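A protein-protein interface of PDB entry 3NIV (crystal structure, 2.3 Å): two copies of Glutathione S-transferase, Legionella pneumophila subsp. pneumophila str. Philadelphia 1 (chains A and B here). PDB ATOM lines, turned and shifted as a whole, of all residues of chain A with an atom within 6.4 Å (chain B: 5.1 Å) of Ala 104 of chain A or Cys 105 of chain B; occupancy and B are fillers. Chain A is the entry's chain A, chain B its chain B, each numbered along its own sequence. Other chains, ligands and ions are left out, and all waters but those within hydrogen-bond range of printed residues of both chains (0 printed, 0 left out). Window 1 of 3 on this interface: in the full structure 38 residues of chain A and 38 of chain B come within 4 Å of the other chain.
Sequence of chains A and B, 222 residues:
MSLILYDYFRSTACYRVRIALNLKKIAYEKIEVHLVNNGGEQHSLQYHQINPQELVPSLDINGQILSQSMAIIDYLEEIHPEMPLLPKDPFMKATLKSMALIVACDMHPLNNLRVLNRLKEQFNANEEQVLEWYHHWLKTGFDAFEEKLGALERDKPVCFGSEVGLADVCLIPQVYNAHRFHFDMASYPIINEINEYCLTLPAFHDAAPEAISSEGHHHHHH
SG of Cys 105 of chain A sits at hydrogen-bond distance from SG of Cys 105 of chain B, at 3.2 Å. NE2 of Gln 68 of chain A is in hydrogen-bond range of OD2 of Asp 106 of chain B (2.9 Å). The side-chain sulfur (SG) of Cys 105 of chain B is in hydrogen-bond range of the backbone carbonyl oxygen (O) of Ala 104 of chain A (3.8 Å). O of Ala 104 of chain B sits at hydrogen-bond distance from SG of Cys 105 of chain A, at 3.6 Å.
The backbone carbonyl oxygen (O) of Leu 101 of chain B is in hydrogen-bond range of the backbone NH (N) of Asp 106 of chain B (3.5 Å). SG of Cys 170 of chain A lies within hydrogen-bond range of SD of Met 70 of chain A.
Among the printed residues, pairs that only touch across the chains: Gln 68 of chain A with Leu 101 of chain B (3.7 Å), Met 70 of chain A with Leu 101 of chain B (3.7 Å), Cys 105 of chain A with Pro 109 of chain B (3.2 Å), Pro 109 of chain A with Cys 105 of chain B (3.4 Å), Pro 109 of chain A with Leu 110 of chain B (3.6 Å) and Arg 114 of chain A with Asp 106 of chain B (3.6 Å).
Of chain B, only Cys 105 (3.8 Å) comes within 4 Å of Ala 104 of chain A. Of chain A, only Ala 104 (3.8 Å), Cys 105 (3.2 Å) and Pro 109 (3.4 Å) come within 4 Å of Cys 105 of chain B. Of the printed residues of chain A, Ala 104 of chain B touches Cys 105. Of the printed residues of chain B, Arg 114 of chain A touches Asp 106. Of the printed residues of chain A, Asp 106 of chain B touches Gln 68 (2.9 Å) and Arg 114 (3.6 Å). Printed residues of chain A within 4 Å of Leu 110 of chain B: Pro 109 (3.6 Å). Printed residues of chain B within 4 Å of Cys 105 of chain A: Ala 104 (3.6 Å), Cys 105 (3.2 Å) and Pro 109 (3.2 Å). Met 99 of chain A touches none of the printed residues of chain B. Ala 100 of chain B touches none of the printed residues of chain A.
Hydrophobic or aromatic side chains of chain B within 4 Å of the printed part of chain A: Leu 101, Pro 109 and Leu 110. Of the 18 printed residues of chain A, 6 touch a printed residue of chain B. Hydrophobic or aromatic side chains of chain A that line the printed part of chain B: Met 70 and Pro 109. Among the printed residues, 10 pairs touch across the chains.
Ala 104 of chain A touches Cys 105 of chain B, and with the chains exchanged Cys 105 of chain A touches Ala 104 of chain B. Cys 105 of chain B touches its own counterpart, Cys 105 of chain A. Cys 105 of chain A touches Pro 109 of chain B, and with the chains exchanged Pro 109 of chain A touches Cys 105 of chain B. Of the 10 pairs that touch across the chains among the printed residues, 5 have their exchanged pair printed and touching as well.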
ATOM      1  N   ARG A  16     -40.073  10.516  -5.849  1.00  0.00           N
ATOM      2  CA  ARG A  16     -39.278   9.324  -5.527  1.00  0.00           C
ATOM      3  C   ARG A  16     -39.458   8.897  -4.082  1.00  0.00           C
ATOM      4  O   ARG A  16     -39.767   7.741  -3.791  1.00  0.00           O
ATOM      5  CB  ARG A  16     -37.795   9.599  -5.715  1.00  0.00           C
ATOM      6  CG  ARG A  16     -37.419  10.086  -7.064  1.00  0.00           C
ATOM      7  CD  ARG A  16     -36.020  10.652  -7.007  1.00  0.00           C
ATOM      8  NE  ARG A  16     -35.698  11.274  -8.278  1.00  0.00           N
ATOM      9  CZ  ARG A  16     -34.616  12.001  -8.488  1.00  0.00           C
ATOM     10  NH1 ARG A  16     -33.763  12.185  -7.494  1.00  0.00           N
ATOM     11  NH2 ARG A  16     -34.397  12.536  -9.683  1.00  0.00           N
ATOM     12  N   GLN A  68     -31.639  15.016   0.567  1.00  0.00           N
ATOM     13  CA  GLN A  68     -31.193  14.271  -0.604  1.00  0.00           C
ATOM     14  C   GLN A  68     -31.972  12.976  -0.767  1.00  0.00           C
ATOM     15  O   GLN A  68     -31.784  12.019  -0.015  1.00  0.00           O
ATOM     16  CB  GLN A  68     -29.688  14.010  -0.579  1.00  0.00           C
ATOM     17  CG  GLN A  68     -28.838  15.264  -0.706  1.00  0.00           C
ATOM     18  CD  GLN A  68     -28.953  15.931  -2.073  1.00  0.00           C
ATOM     19  OE1 GLN A  68     -29.242  15.280  -3.075  1.00  0.00           O
ATOM     20  NE2 GLN A  68     -28.710  17.234  -2.118  1.00  0.00           N
ATOM     21  N   SER A  69     -32.836  12.957  -1.774  1.00  0.00           N
ATOM     22  CA  SER A  69     -33.754  11.846  -2.002  1.00  0.00           C
ATOM     23  C   SER A  69     -33.076  10.479  -2.068  1.00  0.00           C
ATOM     24  O   SER A  69     -33.576   9.519  -1.482  1.00  0.00           O
ATOM     25  CB  SER A  69     -34.617  12.102  -3.250  1.00  0.00           C
ATOM     26  OG  SER A  69     -33.823  12.312  -4.407  1.00  0.00           O
ATOM     27  N   MET A  70     -31.950  10.379  -2.768  1.00  0.00           N
ATOM     28  CA  MET A  70     -31.222   9.107  -2.822  1.00  0.00           C
ATOM     29  C   MET A  70     -30.689   8.701  -1.444  1.00  0.00           C
ATOM     30  O   MET A  70     -30.753   7.533  -1.064  1.00  0.00           O
ATOM     31  CB  MET A  70     -30.090   9.160  -3.844  1.00  0.00           C
ATOM     32  CG  MET A  70     -30.550   9.581  -5.219  1.00  0.00           C
ATOM     33  SD  MET A  70     -32.052   8.496  -5.877  1.00  0.00           S
ATOM     34  CE  MET A  70     -31.059   6.873  -6.347  1.00  0.00           C
ATOM     35  N   MET A  99     -28.373   2.906 -12.576  1.00  0.00           N
ATOM     36  CA  MET A  99     -29.435   3.279 -13.493  1.00  0.00           C
ATOM     37  C   MET A  99     -30.295   4.352 -12.861  1.00  0.00           C
ATOM     38  O   MET A  99     -30.712   5.284 -13.519  1.00  0.00           O
ATOM     39  CB  MET A  99     -30.254   2.058 -13.881  1.00  0.00           C
ATOM     40  CG  MET A  99     -29.480   1.141 -14.799  1.00  0.00           C
ATOM     41  SD  MET A  99     -30.348  -0.573 -15.033  1.00  0.00           S
ATOM     42  CE  MET A  99     -31.998   0.051 -15.922  1.00  0.00           C
ATOM     43  N   ALA A 100     -30.532   4.215 -11.565  1.00  0.00           N
ATOM     44  CA  ALA A 100     -31.196   5.253 -10.809  1.00  0.00           C
ATOM     45  C   ALA A 100     -30.367   6.544 -10.829  1.00  0.00           C
ATOM     46  O   ALA A 100     -30.917   7.636 -10.820  1.00  0.00           O
ATOM     47  CB  ALA A 100     -31.435   4.793  -9.397  1.00  0.00           C
ATOM     48  N   LEU A 101     -29.045   6.415 -10.878  1.00  0.00           N
ATOM     49  CA  LEU A 101     -28.169   7.585 -10.927  1.00  0.00           C
ATOM     50  C   LEU A 101     -28.222   8.282 -12.283  1.00  0.00           C
ATOM     51  O   LEU A 101     -28.126   9.509 -12.376  1.00  0.00           O
ATOM     52  CB  LEU A 101     -26.730   7.189 -10.598  1.00  0.00           C
ATOM     53  CG  LEU A 101     -26.560   6.622  -9.181  1.00  0.00           C
ATOM     54  CD1 LEU A 101     -25.114   6.160  -8.894  1.00  0.00           C
ATOM     55  CD2 LEU A 101     -27.045   7.624  -8.141  1.00  0.00           C
ATOM     56  N   ILE A 102     -28.369   7.493 -13.340  1.00  0.00           N
ATOM     57  CA  ILE A 102     -28.531   8.066 -14.664  1.00  0.00           C
ATOM     58  C   ILE A 102     -29.650   9.114 -14.648  1.00  0.00           C
ATOM     59  O   ILE A 102     -29.558  10.146 -15.295  1.00  0.00           O
ATOM     60  CB  ILE A 102     -28.877   6.995 -15.675  1.00  0.00           C
ATOM     61  CG1 ILE A 102     -27.641   6.148 -15.979  1.00  0.00           C
ATOM     62  CG2 ILE A 102     -29.481   7.632 -16.945  1.00  0.00           C
ATOM     63  CD1 ILE A 102     -27.843   5.126 -17.094  1.00  0.00           C
ATOM     64  N   VAL A 103     -30.702   8.836 -13.892  1.00  0.00           N
ATOM     65  CA  VAL A 103     -31.845   9.730 -13.828  1.00  0.00           C
ATOM     66  C   VAL A 103     -31.543  10.850 -12.867  1.00  0.00           C
ATOM     67  O   VAL A 103     -31.695  12.015 -13.185  1.00  0.00           O
ATOM     68  CB  VAL A 103     -33.094   8.994 -13.304  1.00  0.00           C
ATOM     69  CG1 VAL A 103     -34.139   9.985 -12.821  1.00  0.00           C
ATOM     70  CG2 VAL A 103     -33.647   8.037 -14.360  1.00  0.00           C
ATOM     71  N   ALA A 104     -31.091  10.473 -11.682  1.00  0.00           N
ATOM     72  CA  ALA A 104     -30.880  11.416 -10.606  1.00  0.00           C
ATOM     73  C   ALA A 104     -29.598  12.247 -10.737  1.00  0.00           C
ATOM     74  O   ALA A 104     -29.459  13.249 -10.054  1.00  0.00           O
ATOM     75  CB  ALA A 104     -30.911  10.688  -9.278  1.00  0.00           C
ATOM     76  N   CYS A 105     -28.675  11.845 -11.603  1.00  0.00           N
ATOM     77  CA  CYS A 105     -27.415  12.584 -11.767  1.00  0.00           C
ATOM     78  C   CYS A 105     -27.238  13.138 -13.166  1.00  0.00           C
ATOM     79  O   CYS A 105     -26.730  14.241 -13.341  1.00  0.00           O
ATOM     80  CB  CYS A 105     -26.202  11.699 -11.454  1.00  0.00           C
ATOM     81  SG  CYS A 105     -25.863  11.467  -9.700  1.00  0.00           S
ATOM     82  N   ASP A 106     -27.640  12.356 -14.162  1.00  0.00           N
ATOM     83  CA  ASP A 106     -27.390  12.709 -15.554  1.00  0.00           C
ATOM     84  C   ASP A 106     -28.606  13.297 -16.234  1.00  0.00           C
ATOM     85  O   ASP A 106     -28.558  13.580 -17.425  1.00  0.00           O
ATOM     86  CB  ASP A 106     -26.930  11.485 -16.357  1.00  0.00           C
ATOM     87  CG  ASP A 106     -25.624  10.893 -15.838  1.00  0.00           C
ATOM     88  OD1 ASP A 106     -25.009  11.487 -14.920  1.00  0.00           O
ATOM     89  OD2 ASP A 106     -25.222   9.825 -16.355  1.00  0.00           O
ATOM     90  N   MET A 107     -29.702  13.456 -15.501  1.00  0.00           N
ATOM     91  CA  MET A 107     -30.927  13.967 -16.120  1.00  0.00           C
ATOM     92  C   MET A 107     -31.606  15.042 -15.275  1.00  0.00           C
ATOM     93  O   MET A 107     -31.665  16.211 -15.666  1.00  0.00           O
ATOM     94  CB  MET A 107     -31.929  12.849 -16.399  1.00  0.00           C
ATOM     95  CG  MET A 107     -31.429  11.693 -17.270  1.00  0.00           C
ATOM     96  SD  MET A 107     -32.908  10.417 -17.710  1.00  0.00           S
ATOM     97  CE  MET A 107     -34.151  11.732 -18.443  1.00  0.00           C
ATOM     98  N   HIS A 108     -32.128  14.651 -14.120  1.00  0.00           N
ATOM     99  CA  HIS A 108     -32.884  15.598 -13.324  1.00  0.00           C
ATOM    100  C   HIS A 108     -32.139  16.901 -13.014  1.00  0.00           C
ATOM    101  O   HIS A 108     -32.695  17.973 -13.201  1.00  0.00           O
ATOM    102  CB  HIS A 108     -33.432  14.975 -12.048  1.00  0.00           C
ATOM    103  CG  HIS A 108     -34.517  15.793 -11.420  1.00  0.00           C
ATOM    104  ND1 HIS A 108     -35.510  16.400 -12.165  1.00  0.00           N
ATOM    105  CD2 HIS A 108     -34.768  16.111 -10.127  1.00  0.00           C
ATOM    106  CE1 HIS A 108     -36.319  17.063 -11.356  1.00  0.00           C
ATOM    107  NE2 HIS A 108     -35.899  16.893 -10.114  1.00  0.00           N
ATOM    108  N   PRO A 109     -30.882  16.814 -12.544  1.00  0.00           N
ATOM    109  CA  PRO A 109     -30.170  18.051 -12.188  1.00  0.00           C
ATOM    110  C   PRO A 109     -30.196  19.102 -13.293  1.00  0.00           C
ATOM    111  O   PRO A 109     -30.372  20.287 -12.998  1.00  0.00           O
ATOM    112  CB  PRO A 109     -28.736  17.577 -11.949  1.00  0.00           C
ATOM    113  CG  PRO A 109     -28.889  16.148 -11.535  1.00  0.00           C
ATOM    114  CD  PRO A 109     -30.084  15.605 -12.259  1.00  0.00           C
ATOM    115  N   ARG A 114     -34.371  25.590 -11.133  1.00  0.00           N
ATOM    116  CA  ARG A 114     -33.252  26.486 -10.890  1.00  0.00           C
ATOM    117  C   ARG A 114     -32.373  26.589 -12.125  1.00  0.00           C
ATOM    118  O   ARG A 114     -31.808  27.643 -12.406  1.00  0.00           O
ATOM    119  CB  ARG A 114     -32.427  26.001  -9.684  1.00  0.00           C
ATOM    120  CG  ARG A 114     -31.264  25.067 -10.069  1.00  0.00           C
ATOM    121  CD  ARG A 114     -30.976  23.908  -9.076  1.00  0.00           C
ATOM    122  NE  ARG A 114     -30.086  24.273  -7.982  1.00  0.00           N
ATOM    123  CZ  ARG A 114     -28.884  23.740  -7.745  1.00  0.00           C
ATOM    124  NH1 ARG A 114     -28.373  22.786  -8.518  1.00  0.00           N
ATOM    125  NH2 ARG A 114     -28.186  24.170  -6.707  1.00  0.00           N
ATOM    126  N   CYS A 170     -37.129   5.628  -9.367  1.00  0.00           N
ATOM    127  CA  CYS A 170     -36.597   6.862  -9.946  1.00  0.00           C
ATOM    128  C   CYS A 170     -37.094   7.113 -11.365  1.00  0.00           C
ATOM    129  O   CYS A 170     -37.147   8.253 -11.815  1.00  0.00           O
ATOM    130  CB  CYS A 170     -35.069   6.874  -9.914  1.00  0.00           C
ATOM    131  SG  CYS A 170     -34.393   6.908  -8.248  1.00  0.00           S
ATOM    132  N   GLN A 174     -39.315  10.603 -13.470  1.00  0.00           N
ATOM    133  CA  GLN A 174     -38.664  11.163 -14.650  1.00  0.00           C
ATOM    134  C   GLN A 174     -39.556  11.151 -15.900  1.00  0.00           C
ATOM    135  O   GLN A 174     -39.544  12.090 -16.687  1.00  0.00           O
ATOM    136  CB  GLN A 174     -37.352  10.432 -14.941  1.00  0.00           C
ATOM    137  CG  GLN A 174     -36.468  11.142 -15.955  1.00  0.00           C
ATOM    138  CD  GLN A 174     -36.133  12.577 -15.551  1.00  0.00           C
ATOM    139  OE1 GLN A 174     -36.411  13.508 -16.293  1.00  0.00           O
ATOM    140  NE2 GLN A 174     -35.539  12.754 -14.368  1.00  0.00           N
ATOM    141  N   ALA B 100     -22.305  13.844   0.034  1.00  0.00           N
ATOM    142  CA  ALA B 100     -21.621  13.348  -1.149  1.00  0.00           C
ATOM    143  C   ALA B 100     -22.483  13.603  -2.380  1.00  0.00           C
ATOM    144  O   ALA B 100     -21.985  13.922  -3.462  1.00  0.00           O
ATOM    145  CB  ALA B 100     -21.311  11.870  -0.999  1.00  0.00           C
ATOM    146  N   LEU B 101     -23.790  13.462  -2.196  1.00  0.00           N
ATOM    147  CA  LEU B 101     -24.754  13.744  -3.257  1.00  0.00           C
ATOM    148  C   LEU B 101     -24.826  15.229  -3.605  1.00  0.00           C
ATOM    149  O   LEU B 101     -25.042  15.572  -4.760  1.00  0.00           O
ATOM    150  CB  LEU B 101     -26.134  13.193  -2.886  1.00  0.00           C
ATOM    151  CG  LEU B 101     -26.088  11.672  -2.737  1.00  0.00           C
ATOM    152  CD1 LEU B 101     -27.384  11.087  -2.173  1.00  0.00           C
ATOM    153  CD2 LEU B 101     -25.745  11.054  -4.081  1.00  0.00           C
ATOM    154  N   ILE B 102     -24.633  16.107  -2.623  1.00  0.00           N
ATOM    155  CA  ILE B 102     -24.569  17.537  -2.927  1.00  0.00           C
ATOM    156  C   ILE B 102     -23.594  17.691  -4.074  1.00  0.00           C
ATOM    157  O   ILE B 102     -23.877  18.365  -5.059  1.00  0.00           O
ATOM    158  CB  ILE B 102     -24.078  18.401  -1.746  1.00  0.00           C
ATOM    159  CG1 ILE B 102     -25.186  18.652  -0.720  1.00  0.00           C
ATOM    160  CG2 ILE B 102     -23.540  19.744  -2.227  1.00  0.00           C
ATOM    161  CD1 ILE B 102     -24.685  19.408   0.517  1.00  0.00           C
ATOM    162  N   VAL B 103     -22.448  17.037  -3.958  1.00  0.00           N
ATOM    163  CA  VAL B 103     -21.416  17.156  -4.975  1.00  0.00           C
ATOM    164  C   VAL B 103     -21.760  16.388  -6.241  1.00  0.00           C
ATOM    165  O   VAL B 103     -21.727  16.932  -7.340  1.00  0.00           O
ATOM    166  CB  VAL B 103     -20.041  16.676  -4.445  1.00  0.00           C
ATOM    167  CG1 VAL B 103     -19.119  16.287  -5.597  1.00  0.00           C
ATOM    168  CG2 VAL B 103     -19.415  17.754  -3.589  1.00  0.00           C
ATOM    169  N   ALA B 104     -22.069  15.111  -6.081  1.00  0.00           N
ATOM    170  CA  ALA B 104     -22.281  14.236  -7.222  1.00  0.00           C
ATOM    171  C   ALA B 104     -23.549  14.585  -8.007  1.00  0.00           C
ATOM    172  O   ALA B 104     -23.650  14.270  -9.183  1.00  0.00           O
ATOM    173  CB  ALA B 104     -22.302  12.762  -6.763  1.00  0.00           C
ATOM    174  N   CYS B 105     -24.502  15.241  -7.354  1.00  0.00           N
ATOM    175  CA  CYS B 105     -25.797  15.516  -7.954  1.00  0.00           C
ATOM    176  C   CYS B 105     -26.081  16.982  -8.217  1.00  0.00           C
ATOM    177  O   CYS B 105     -26.606  17.329  -9.263  1.00  0.00           O
ATOM    178  CB  CYS B 105     -26.903  14.958  -7.075  1.00  0.00           C
ATOM    179  SG  CYS B 105     -27.014  13.191  -7.208  1.00  0.00           S
ATOM    180  N   ASP B 106     -25.744  17.839  -7.266  1.00  0.00           N
ATOM    181  CA  ASP B 106     -26.112  19.244  -7.343  1.00  0.00           C
ATOM    182  C   ASP B 106     -24.992  20.109  -7.885  1.00  0.00           C
ATOM    183  O   ASP B 106     -25.155  21.316  -8.013  1.00  0.00           O
ATOM    184  CB  ASP B 106     -26.514  19.753  -5.961  1.00  0.00           C
ATOM    185  CG  ASP B 106     -27.660  18.959  -5.362  1.00  0.00           C
ATOM    186  OD1 ASP B 106     -28.293  18.180  -6.114  1.00  0.00           O
ATOM    187  OD2 ASP B 106     -27.926  19.116  -4.149  1.00  0.00           O
ATOM    188  N   MET B 107     -23.857  19.496  -8.201  1.00  0.00           N
ATOM    189  CA  MET B 107     -22.683  20.258  -8.631  1.00  0.00           C
ATOM    190  C   MET B 107     -22.086  19.731  -9.927  1.00  0.00           C
ATOM    191  O   MET B 107     -22.248  20.309 -10.989  1.00  0.00           O
ATOM    192  CB  MET B 107     -21.607  20.261  -7.534  1.00  0.00           C
ATOM    193  CG  MET B 107     -22.035  20.941  -6.242  1.00  0.00           C
ATOM    194  SD  MET B 107     -20.589  21.160  -4.879  1.00  0.00           S
ATOM    195  CE  MET B 107     -19.420  22.345  -5.894  1.00  0.00           C
ATOM    196  N   PRO B 109     -22.776  17.480 -12.157  1.00  0.00           N
ATOM    197  CA  PRO B 109     -23.482  17.338 -13.442  1.00  0.00           C
ATOM    198  C   PRO B 109     -23.663  18.661 -14.208  1.00  0.00           C
ATOM    199  O   PRO B 109     -23.507  18.663 -15.429  1.00  0.00           O
ATOM    200  CB  PRO B 109     -24.838  16.743 -13.042  1.00  0.00           C
ATOM    201  CG  PRO B 109     -24.593  16.081 -11.739  1.00  0.00           C
ATOM    202  CD  PRO B 109     -23.539  16.907 -11.039  1.00  0.00           C
ATOM    203  N   LEU B 110     -23.957  19.754 -13.500  1.00  0.00           N
ATOM    204  CA  LEU B 110     -24.232  21.054 -14.131  1.00  0.00           C
ATOM    205  C   LEU B 110     -23.009  21.634 -14.838  1.00  0.00           C
ATOM    206  O   LEU B 110     -23.126  22.455 -15.752  1.00  0.00           O
ATOM    207  CB  LEU B 110     -24.747  22.069 -13.101  1.00  0.00           C
ATOM    208  CG  LEU B 110     -26.117  21.873 -12.447  1.00  0.00           C
ATOM    209  CD1 LEU B 110     -27.213  21.926 -13.482  1.00  0.00           C
ATOM    210  CD2 LEU B 110     -26.154  20.550 -11.720  1.00  0.00           C
